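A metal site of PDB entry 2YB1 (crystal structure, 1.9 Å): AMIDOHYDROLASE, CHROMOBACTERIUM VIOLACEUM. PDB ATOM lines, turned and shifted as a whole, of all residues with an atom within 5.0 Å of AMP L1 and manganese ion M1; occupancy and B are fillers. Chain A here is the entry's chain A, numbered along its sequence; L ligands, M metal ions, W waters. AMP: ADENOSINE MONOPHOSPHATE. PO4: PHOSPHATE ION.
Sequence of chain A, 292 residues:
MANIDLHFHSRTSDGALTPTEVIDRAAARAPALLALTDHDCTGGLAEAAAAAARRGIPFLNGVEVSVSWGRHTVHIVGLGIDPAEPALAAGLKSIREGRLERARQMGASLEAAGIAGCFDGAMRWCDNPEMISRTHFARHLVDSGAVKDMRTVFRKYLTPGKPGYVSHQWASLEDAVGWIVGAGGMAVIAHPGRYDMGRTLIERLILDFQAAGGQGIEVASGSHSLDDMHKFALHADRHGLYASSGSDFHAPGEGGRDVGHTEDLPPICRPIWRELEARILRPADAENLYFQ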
ATOM      1  N   HIS A   9     -24.237  19.713  12.115  1.00  0.00           N
ATOM      2  CA  HIS A   9     -24.496  18.840  13.254  1.00  0.00           C
ATOM      3  C   HIS A   9     -23.364  18.824  14.266  1.00  0.00           C
ATOM      4  O   HIS A   9     -22.236  19.208  13.952  1.00  0.00           O
ATOM      5  CB  HIS A   9     -24.758  17.405  12.780  1.00  0.00           C
ATOM      6  CG  HIS A   9     -25.988  17.297  11.942  1.00  0.00           C
ATOM      7  ND1 HIS A   9     -27.214  16.949  12.477  1.00  0.00           N
ATOM      8  CD2 HIS A   9     -26.203  17.548  10.637  1.00  0.00           C
ATOM      9  CE1 HIS A   9     -28.119  16.971  11.519  1.00  0.00           C
ATOM     10  NE2 HIS A   9     -27.536  17.329  10.399  1.00  0.00           N
ATOM     11  N   ASP A  14     -25.803  13.499  15.543  1.00  0.00           N
ATOM     12  CA  ASP A  14     -24.883  12.678  14.744  1.00  0.00           C
ATOM     13  C   ASP A  14     -23.578  13.296  14.222  1.00  0.00           C
ATOM     14  O   ASP A  14     -22.889  12.687  13.405  1.00  0.00           O
ATOM     15  CB  ASP A  14     -25.610  11.819  13.692  1.00  0.00           C
ATOM     16  CG  ASP A  14     -26.144  12.644  12.563  1.00  0.00           C
ATOM     17  OD1 ASP A  14     -26.119  13.883  12.672  1.00  0.00           O
ATOM     18  OD2 ASP A  14     -26.582  12.038  11.570  1.00  0.00           O
ATOM     19  N   HIS A  39     -30.372  16.770  14.796  1.00  0.00           N
ATOM     20  CA  HIS A  39     -31.571  15.955  14.583  1.00  0.00           C
ATOM     21  C   HIS A  39     -32.433  15.873  15.830  1.00  0.00           C
ATOM     22  O   HIS A  39     -31.944  15.478  16.889  1.00  0.00           O
ATOM     23  CB  HIS A  39     -31.166  14.525  14.220  1.00  0.00           C
ATOM     24  CG  HIS A  39     -30.476  14.393  12.898  1.00  0.00           C
ATOM     25  ND1 HIS A  39     -31.151  14.507  11.703  1.00  0.00           N
ATOM     26  CD2 HIS A  39     -29.195  14.119  12.590  1.00  0.00           C
ATOM     27  CE1 HIS A  39     -30.300  14.311  10.705  1.00  0.00           C
ATOM     28  NE2 HIS A  39     -29.107  14.078  11.213  1.00  0.00           N
ATOM     29  N   SER A  66     -37.164  14.971  11.980  1.00  0.00           N
ATOM     30  CA  SER A  66     -37.445  13.766  11.189  1.00  0.00           C
ATOM     31  C   SER A  66     -38.950  13.631  10.975  1.00  0.00           C
ATOM     32  O   SER A  66     -39.732  13.702  11.923  1.00  0.00           O
ATOM     33  CB  SER A  66     -36.947  12.517  11.919  1.00  0.00           C
ATOM     34  OG  SER A  66     -35.571  12.620  12.277  1.00  0.00           O
ATOM     35  N   HIS A  75     -36.728  15.470   5.940  1.00  0.00           N
ATOM     36  CA  HIS A  75     -36.202  16.236   7.060  1.00  0.00           C
ATOM     37  C   HIS A  75     -36.582  17.703   6.943  1.00  0.00           C
ATOM     38  O   HIS A  75     -36.380  18.320   5.891  1.00  0.00           O
ATOM     39  CB  HIS A  75     -34.681  16.078   7.147  1.00  0.00           C
ATOM     40  CG  HIS A  75     -34.243  14.733   7.628  1.00  0.00           C
ATOM     41  ND1 HIS A  75     -32.941  14.290   7.550  1.00  0.00           N
ATOM     42  CD2 HIS A  75     -34.939  13.723   8.211  1.00  0.00           C
ATOM     43  CE1 HIS A  75     -32.845  13.081   8.063  1.00  0.00           C
ATOM     44  NE2 HIS A  75     -34.046  12.720   8.483  1.00  0.00           N
ATOM     45  N   ARG A  99     -36.108   5.810  19.418  1.00  0.00           N
ATOM     46  CA  ARG A  99     -34.803   5.760  18.765  1.00  0.00           C
ATOM     47  C   ARG A  99     -33.916   4.630  19.297  1.00  0.00           C
ATOM     48  O   ARG A  99     -33.348   3.851  18.523  1.00  0.00           O
ATOM     49  CB  ARG A  99     -34.108   7.121  18.880  1.00  0.00           C
ATOM     50  CG  ARG A  99     -33.179   7.461  17.737  1.00  0.00           C
ATOM     51  CD  ARG A  99     -32.827   8.939  17.719  1.00  0.00           C
ATOM     52  NE  ARG A  99     -33.313   9.628  16.511  1.00  0.00           N
ATOM     53  CZ  ARG A  99     -32.924   9.336  15.271  1.00  0.00           C
ATOM     54  NH1 ARG A  99     -32.049   8.359  15.041  1.00  0.00           N
ATOM     55  NH2 ARG A  99     -33.425  10.019  14.232  1.00  0.00           N
ATOM     56  N   ARG A 102     -35.321   1.138  18.354  1.00  0.00           N
ATOM     57  CA  ARG A 102     -35.049   0.900  16.945  1.00  0.00           C
ATOM     58  C   ARG A 102     -33.597   0.502  16.710  1.00  0.00           C
ATOM     59  O   ARG A 102     -33.286  -0.369  15.882  1.00  0.00           O
ATOM     60  CB  ARG A 102     -35.382   2.157  16.155  1.00  0.00           C
ATOM     61  CG  ARG A 102     -34.977   2.172  14.675  1.00  0.00           C
ATOM     62  CD  ARG A 102     -35.384   3.554  14.112  1.00  0.00           C
ATOM     63  NE  ARG A 102     -35.026   3.813  12.719  1.00  0.00           N
ATOM     64  CZ  ARG A 102     -34.003   4.577  12.337  1.00  0.00           C
ATOM     65  NH1 ARG A 102     -33.208   5.153  13.250  1.00  0.00           N
ATOM     66  NH2 ARG A 102     -33.778   4.777  11.037  1.00  0.00           N
ATOM     67  N   ILE A 132     -29.122   7.910  19.246  1.00  0.00           N
ATOM     68  CA  ILE A 132     -28.460   6.885  18.441  1.00  0.00           C
ATOM     69  C   ILE A 132     -29.035   6.811  17.008  1.00  0.00           C
ATOM     70  O   ILE A 132     -30.257   6.758  16.819  1.00  0.00           O
ATOM     71  CB  ILE A 132     -28.521   5.488  19.151  1.00  0.00           C
ATOM     72  CG1 ILE A 132     -27.773   4.413  18.359  1.00  0.00           C
ATOM     73  CG2 ILE A 132     -29.980   5.055  19.413  1.00  0.00           C
ATOM     74  CD1 ILE A 132     -26.246   4.554  18.368  1.00  0.00           C
ATOM     75  N   SER A 133     -28.155   6.787  16.023  1.00  0.00           N
ATOM     76  CA  SER A 133     -28.536   7.051  14.630  1.00  0.00           C
ATOM     77  C   SER A 133     -27.866   6.067  13.666  1.00  0.00           C
ATOM     78  O   SER A 133     -26.835   5.503  13.993  1.00  0.00           O
ATOM     79  CB  SER A 133     -28.087   8.478  14.299  1.00  0.00           C
ATOM     80  OG  SER A 133     -27.905   8.703  12.921  1.00  0.00           O
ATOM     81  N   ARG A 134     -28.457   5.860  12.485  1.00  0.00           N
ATOM     82  CA  ARG A 134     -27.817   5.094  11.422  1.00  0.00           C
ATOM     83  C   ARG A 134     -26.408   5.626  11.152  1.00  0.00           C
ATOM     84  O   ARG A 134     -25.541   4.866  10.703  1.00  0.00           O
ATOM     85  CB  ARG A 134     -28.622   5.143  10.114  1.00  0.00           C
ATOM     86  CG  ARG A 134     -29.930   4.354  10.169  1.00  0.00           C
ATOM     87  CD  ARG A 134     -30.606   4.276   8.798  1.00  0.00           C
ATOM     88  NE  ARG A 134     -31.249   5.537   8.435  1.00  0.00           N
ATOM     89  CZ  ARG A 134     -31.509   5.912   7.187  1.00  0.00           C
ATOM     90  NH1 ARG A 134     -31.179   5.125   6.167  1.00  0.00           N
ATOM     91  NH2 ARG A 134     -32.107   7.078   6.953  1.00  0.00           N
ATOM     92  N   THR A 135     -26.190   6.912  11.395  1.00  0.00           N
ATOM     93  CA  THR A 135     -24.870   7.523  11.171  1.00  0.00           C
ATOM     94  C   THR A 135     -23.822   6.875  12.059  1.00  0.00           C
ATOM     95  O   THR A 135     -22.721   6.582  11.605  1.00  0.00           O
ATOM     96  CB  THR A 135     -24.890   9.042  11.454  1.00  0.00           C
ATOM     97  OG1 THR A 135     -25.852   9.672  10.595  1.00  0.00           O
ATOM     98  CG2 THR A 135     -23.508   9.671  11.212  1.00  0.00           C
ATOM     99  N   MET A 150     -18.323   5.224   4.082  1.00  0.00           N
ATOM    100  CA  MET A 150     -19.701   5.591   4.437  1.00  0.00           C
ATOM    101  C   MET A 150     -20.661   5.335   3.281  1.00  0.00           C
ATOM    102  O   MET A 150     -21.793   4.873   3.491  1.00  0.00           O
ATOM    103  CB  MET A 150     -19.787   7.062   4.858  1.00  0.00           C
ATOM    104  CG  MET A 150     -19.009   7.411   6.123  1.00  0.00           C
ATOM    105  SD  MET A 150     -19.804   6.873   7.651  1.00  0.00           S
ATOM    106  CE  MET A 150     -21.107   8.107   7.835  1.00  0.00           C
ATOM    107  N   PHE A 154     -24.216   2.460   3.115  1.00  0.00           N
ATOM    108  CA  PHE A 154     -25.631   2.674   2.842  1.00  0.00           C
ATOM    109  C   PHE A 154     -26.082   2.031   1.541  1.00  0.00           C
ATOM    110  O   PHE A 154     -27.276   1.885   1.268  1.00  0.00           O
ATOM    111  CB  PHE A 154     -25.954   4.179   2.892  1.00  0.00           C
ATOM    112  CG  PHE A 154     -25.897   4.746   4.286  1.00  0.00           C
ATOM    113  CD1 PHE A 154     -27.009   4.686   5.113  1.00  0.00           C
ATOM    114  CD2 PHE A 154     -24.721   5.287   4.778  1.00  0.00           C
ATOM    115  CE1 PHE A 154     -26.946   5.181   6.411  1.00  0.00           C
ATOM    116  CE2 PHE A 154     -24.659   5.782   6.076  1.00  0.00           C
ATOM    117  CZ  PHE A 154     -25.773   5.735   6.896  1.00  0.00           C
ATOM    118  N   TRP A 170     -41.780   8.619  11.983  1.00  0.00           N
ATOM    119  CA  TRP A 170     -41.341   9.853  12.631  1.00  0.00           C
ATOM    120  C   TRP A 170     -42.514  10.840  12.735  1.00  0.00           C
ATOM    121  O   TRP A 170     -43.673  10.431  12.693  1.00  0.00           O
ATOM    122  CB  TRP A 170     -40.138  10.457  11.894  1.00  0.00           C
ATOM    123  CG  TRP A 170     -39.043   9.472  11.646  1.00  0.00           C
ATOM    124  CD1 TRP A 170     -38.759   8.849  10.459  1.00  0.00           C
ATOM    125  CD2 TRP A 170     -38.088   8.981  12.593  1.00  0.00           C
ATOM    126  NE1 TRP A 170     -37.672   8.012  10.618  1.00  0.00           N
ATOM    127  CE2 TRP A 170     -37.250   8.076  11.914  1.00  0.00           C
ATOM    128  CE3 TRP A 170     -37.854   9.232  13.948  1.00  0.00           C
ATOM    129  CZ2 TRP A 170     -36.183   7.407  12.546  1.00  0.00           C
ATOM    130  CZ3 TRP A 170     -36.794   8.566  14.587  1.00  0.00           C
ATOM    131  CH2 TRP A 170     -35.974   7.672  13.873  1.00  0.00           C
ATOM    132  N   ARG A 194     -32.062  14.922  -2.244  1.00  0.00           N
ATOM    133  CA  ARG A 194     -31.802  13.575  -1.731  1.00  0.00           C
ATOM    134  C   ARG A 194     -33.037  12.675  -1.781  1.00  0.00           C
ATOM    135  O   ARG A 194     -32.926  11.458  -1.673  1.00  0.00           O
ATOM    136  CB  ARG A 194     -31.277  13.605  -0.288  1.00  0.00           C
ATOM    137  CG  ARG A 194     -29.925  14.258  -0.104  1.00  0.00           C
ATOM    138  CD  ARG A 194     -28.960  13.319   0.635  1.00  0.00           C
ATOM    139  NE  ARG A 194     -29.543  12.692   1.828  1.00  0.00           N
ATOM    140  CZ  ARG A 194     -29.175  12.969   3.088  1.00  0.00           C
ATOM    141  NH1 ARG A 194     -28.236  13.875   3.324  1.00  0.00           N
ATOM    142  NH2 ARG A 194     -29.756  12.334   4.103  1.00  0.00           N
ATOM    143  N   HIS A 250     -21.077  17.034   9.092  1.00  0.00           N
ATOM    144  CA  HIS A 250     -21.112  16.056  10.193  1.00  0.00           C
ATOM    145  C   HIS A 250     -19.723  15.863  10.771  1.00  0.00           C
ATOM    146  O   HIS A 250     -19.531  15.914  11.984  1.00  0.00           O
ATOM    147  CB  HIS A 250     -21.660  14.688   9.754  1.00  0.00           C
ATOM    148  CG  HIS A 250     -23.133  14.660   9.548  1.00  0.00           C
ATOM    149  ND1 HIS A 250     -23.754  15.319   8.505  1.00  0.00           N
ATOM    150  CD2 HIS A 250     -24.120  14.041  10.238  1.00  0.00           C
ATOM    151  CE1 HIS A 250     -25.057  15.107   8.559  1.00  0.00           C
ATOM    152  NE2 HIS A 250     -25.304  14.335   9.606  1.00  0.00           N
HETATM  153  P   AMP L   1     -31.559   7.959  11.392  1.00  0.00           P
HETATM  154  O1P AMP L   1     -32.371   7.224  10.348  1.00  0.00           O
HETATM  155  O2P AMP L   1     -32.252   9.279  11.678  1.00  0.00           O
HETATM  156  O3P AMP L   1     -31.273   7.042  12.560  1.00  0.00           O
HETATM  157  O5' AMP L   1     -30.209   8.229  10.592  1.00  0.00           O
HETATM  158  C5' AMP L   1     -30.203   9.071   9.453  1.00  0.00           C
HETATM  159  C4' AMP L   1     -28.856   9.723   9.254  1.00  0.00           C
HETATM  160  O4' AMP L   1     -27.970   8.784   8.601  1.00  0.00           O
HETATM  161  C3' AMP L   1     -28.853  10.941   8.339  1.00  0.00           C
HETATM  162  O3' AMP L   1     -29.219  12.133   9.012  1.00  0.00           O
HETATM  163  C2' AMP L   1     -27.420  10.970   7.793  1.00  0.00           C
HETATM  164  O2' AMP L   1     -26.554  11.602   8.725  1.00  0.00           O
HETATM  165  C1' AMP L   1     -27.076   9.478   7.745  1.00  0.00           C
HETATM  166  N9  AMP L   1     -27.215   8.934   6.378  1.00  0.00           N
HETATM  167  C8  AMP L   1     -28.349   8.455   5.821  1.00  0.00           C
HETATM  168  N7  AMP L   1     -28.117   8.049   4.542  1.00  0.00           N
HETATM  169  C5  AMP L   1     -26.811   8.275   4.276  1.00  0.00           C
HETATM  170  C6  AMP L   1     -25.895   8.073   3.130  1.00  0.00           C
HETATM  171  N6  AMP L   1     -26.343   7.540   1.965  1.00  0.00           N
HETATM  172  N1  AMP L   1     -24.600   8.437   3.271  1.00  0.00           N
HETATM  173  C2  AMP L   1     -24.135   8.976   4.424  1.00  0.00           C
HETATM  174  N3  AMP L   1     -24.902   9.183   5.509  1.00  0.00           N
HETATM  175  C4  AMP L   1     -26.220   8.852   5.490  1.00  0.00           C
HETATM  176  P   PO4 L   2     -28.722  14.739   7.176  1.00  0.00           P
HETATM  177  O1  PO4 L   2     -27.718  14.294   6.135  1.00  0.00           O
HETATM  178  O2  PO4 L   2     -28.047  14.799   8.511  1.00  0.00           O
HETATM  179  O3  PO4 L   2     -29.239  16.128   6.860  1.00  0.00           O
HETATM  180  O4  PO4 L   2     -29.873  13.764   7.186  1.00  0.00           O
HETATM  181 MN    MN M   1     -27.342  13.418  10.065  1.00  0.00          MN
HETATM  182 MN    MN M   2     -28.609  17.276   8.526  1.00  0.00          MN
HETATM  183 MN    MN M   3     -31.284  15.563   6.776  1.00  0.00          MN
HETATM  184  O   HOH W   1     -29.707  10.817  12.902  1.00  0.00           O
HETATM  185  O   HOH W   2     -34.217  10.770  10.449  1.00  0.00           O
HETATM  186  O   HOH W   3     -24.355  11.409   7.419  1.00  0.00           O
HETATM  187  O   HOH W   4     -34.508   8.230   9.160  1.00  0.00           O
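The guanidinium group (NH1) of Arg 102 is in salt-bridge range of an oxygen (O3P) of AMP L1.
OG1 of Thr 135 sits at hydrogen-bond distance from O4' of AMP L1 (3.0 Å).
The backbone NH (N) of Arg 134 sits at hydrogen-bond distance from an oxygen (O3P) of AMP L1, 3.1 Å away.
NE of Arg 134 lies within salt-bridge range of O1P of AMP L1, 2.8 Å away.
The guanidinium group of Arg 99 lies within salt-bridge range of an oxygen (O2P) of AMP L1.
The side-chain hydroxyl of Ser 133 sits at hydrogen-bond distance from an oxygen (O5') of AMP L1.
The side-chain carboxylate of Asp 14 sits close to the side-chain hydroxyl of Thr 135.
The backbone NH (N) of Thr 135 sits at hydrogen-bond distance from the side-chain hydroxyl (OG) of Ser 133, 2.9 Å away.
The side-chain carboxylate (OD1) of Asp 14 lies within hydrogen-bond range of a ring nitrogen (ND1) of His 9 (3.3 Å).
The guanidinium group (NH1) of Arg 99 is in hydrogen-bond range of the backbone carbonyl oxygen (O) of Ile 132 (3.0 Å).
Merely in contact with AMP L1: His 75 (3.9 Å) and Phe 154 (3.4 Å).
Ten residues have an atom within 4 Å of AMP L1: Asp 14, His 39, His 75, Arg 99, Arg 102, Ser 133, Arg 134, Thr 135, Phe 154 and His 250.
The nearest printed residue that does not touch AMP L1 is Ile 132 (4.4 Å).
Merely in contact with manganese ion M1: His 9 (3.9 Å).
Within 4 Å of manganese ion M1: His 9, Asp 14, His 39 and His 250.
Manganese ion M1 is bound by the side-chain carboxylate of Asp 14 (2.2 Å), an oxygen (O2) of PO4 L2 (2.2 Å), a ring nitrogen (NE2) of His 39 (2.2 Å), a ring nitrogen (NE2) of His 250 (2.3 Å), an oxygen (O2') of AMP L1 (2.4 Å) and an oxygen (O3') of AMP L1 (2.5 Å).
Slightly farther from manganese ion M1 lies the side-chain carboxylate (OD1) of Asp 14 (2.9 Å).
Water W4 lies within hydrogen-bond range of O1P of AMP L1, NH2 of Arg 134 and NE1 of Trp 170.
Water W2 lies within hydrogen-bond range of an oxygen (O2P) of AMP L1, a ring nitrogen (NE2) of His 75 and the side-chain hydroxyl of Ser 66.
Water W1 bridges the side-chain hydroxyl (OG) of Ser 133 (2.8 Å) and an oxygen (O2P) of AMP L1 (3.2 Å).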
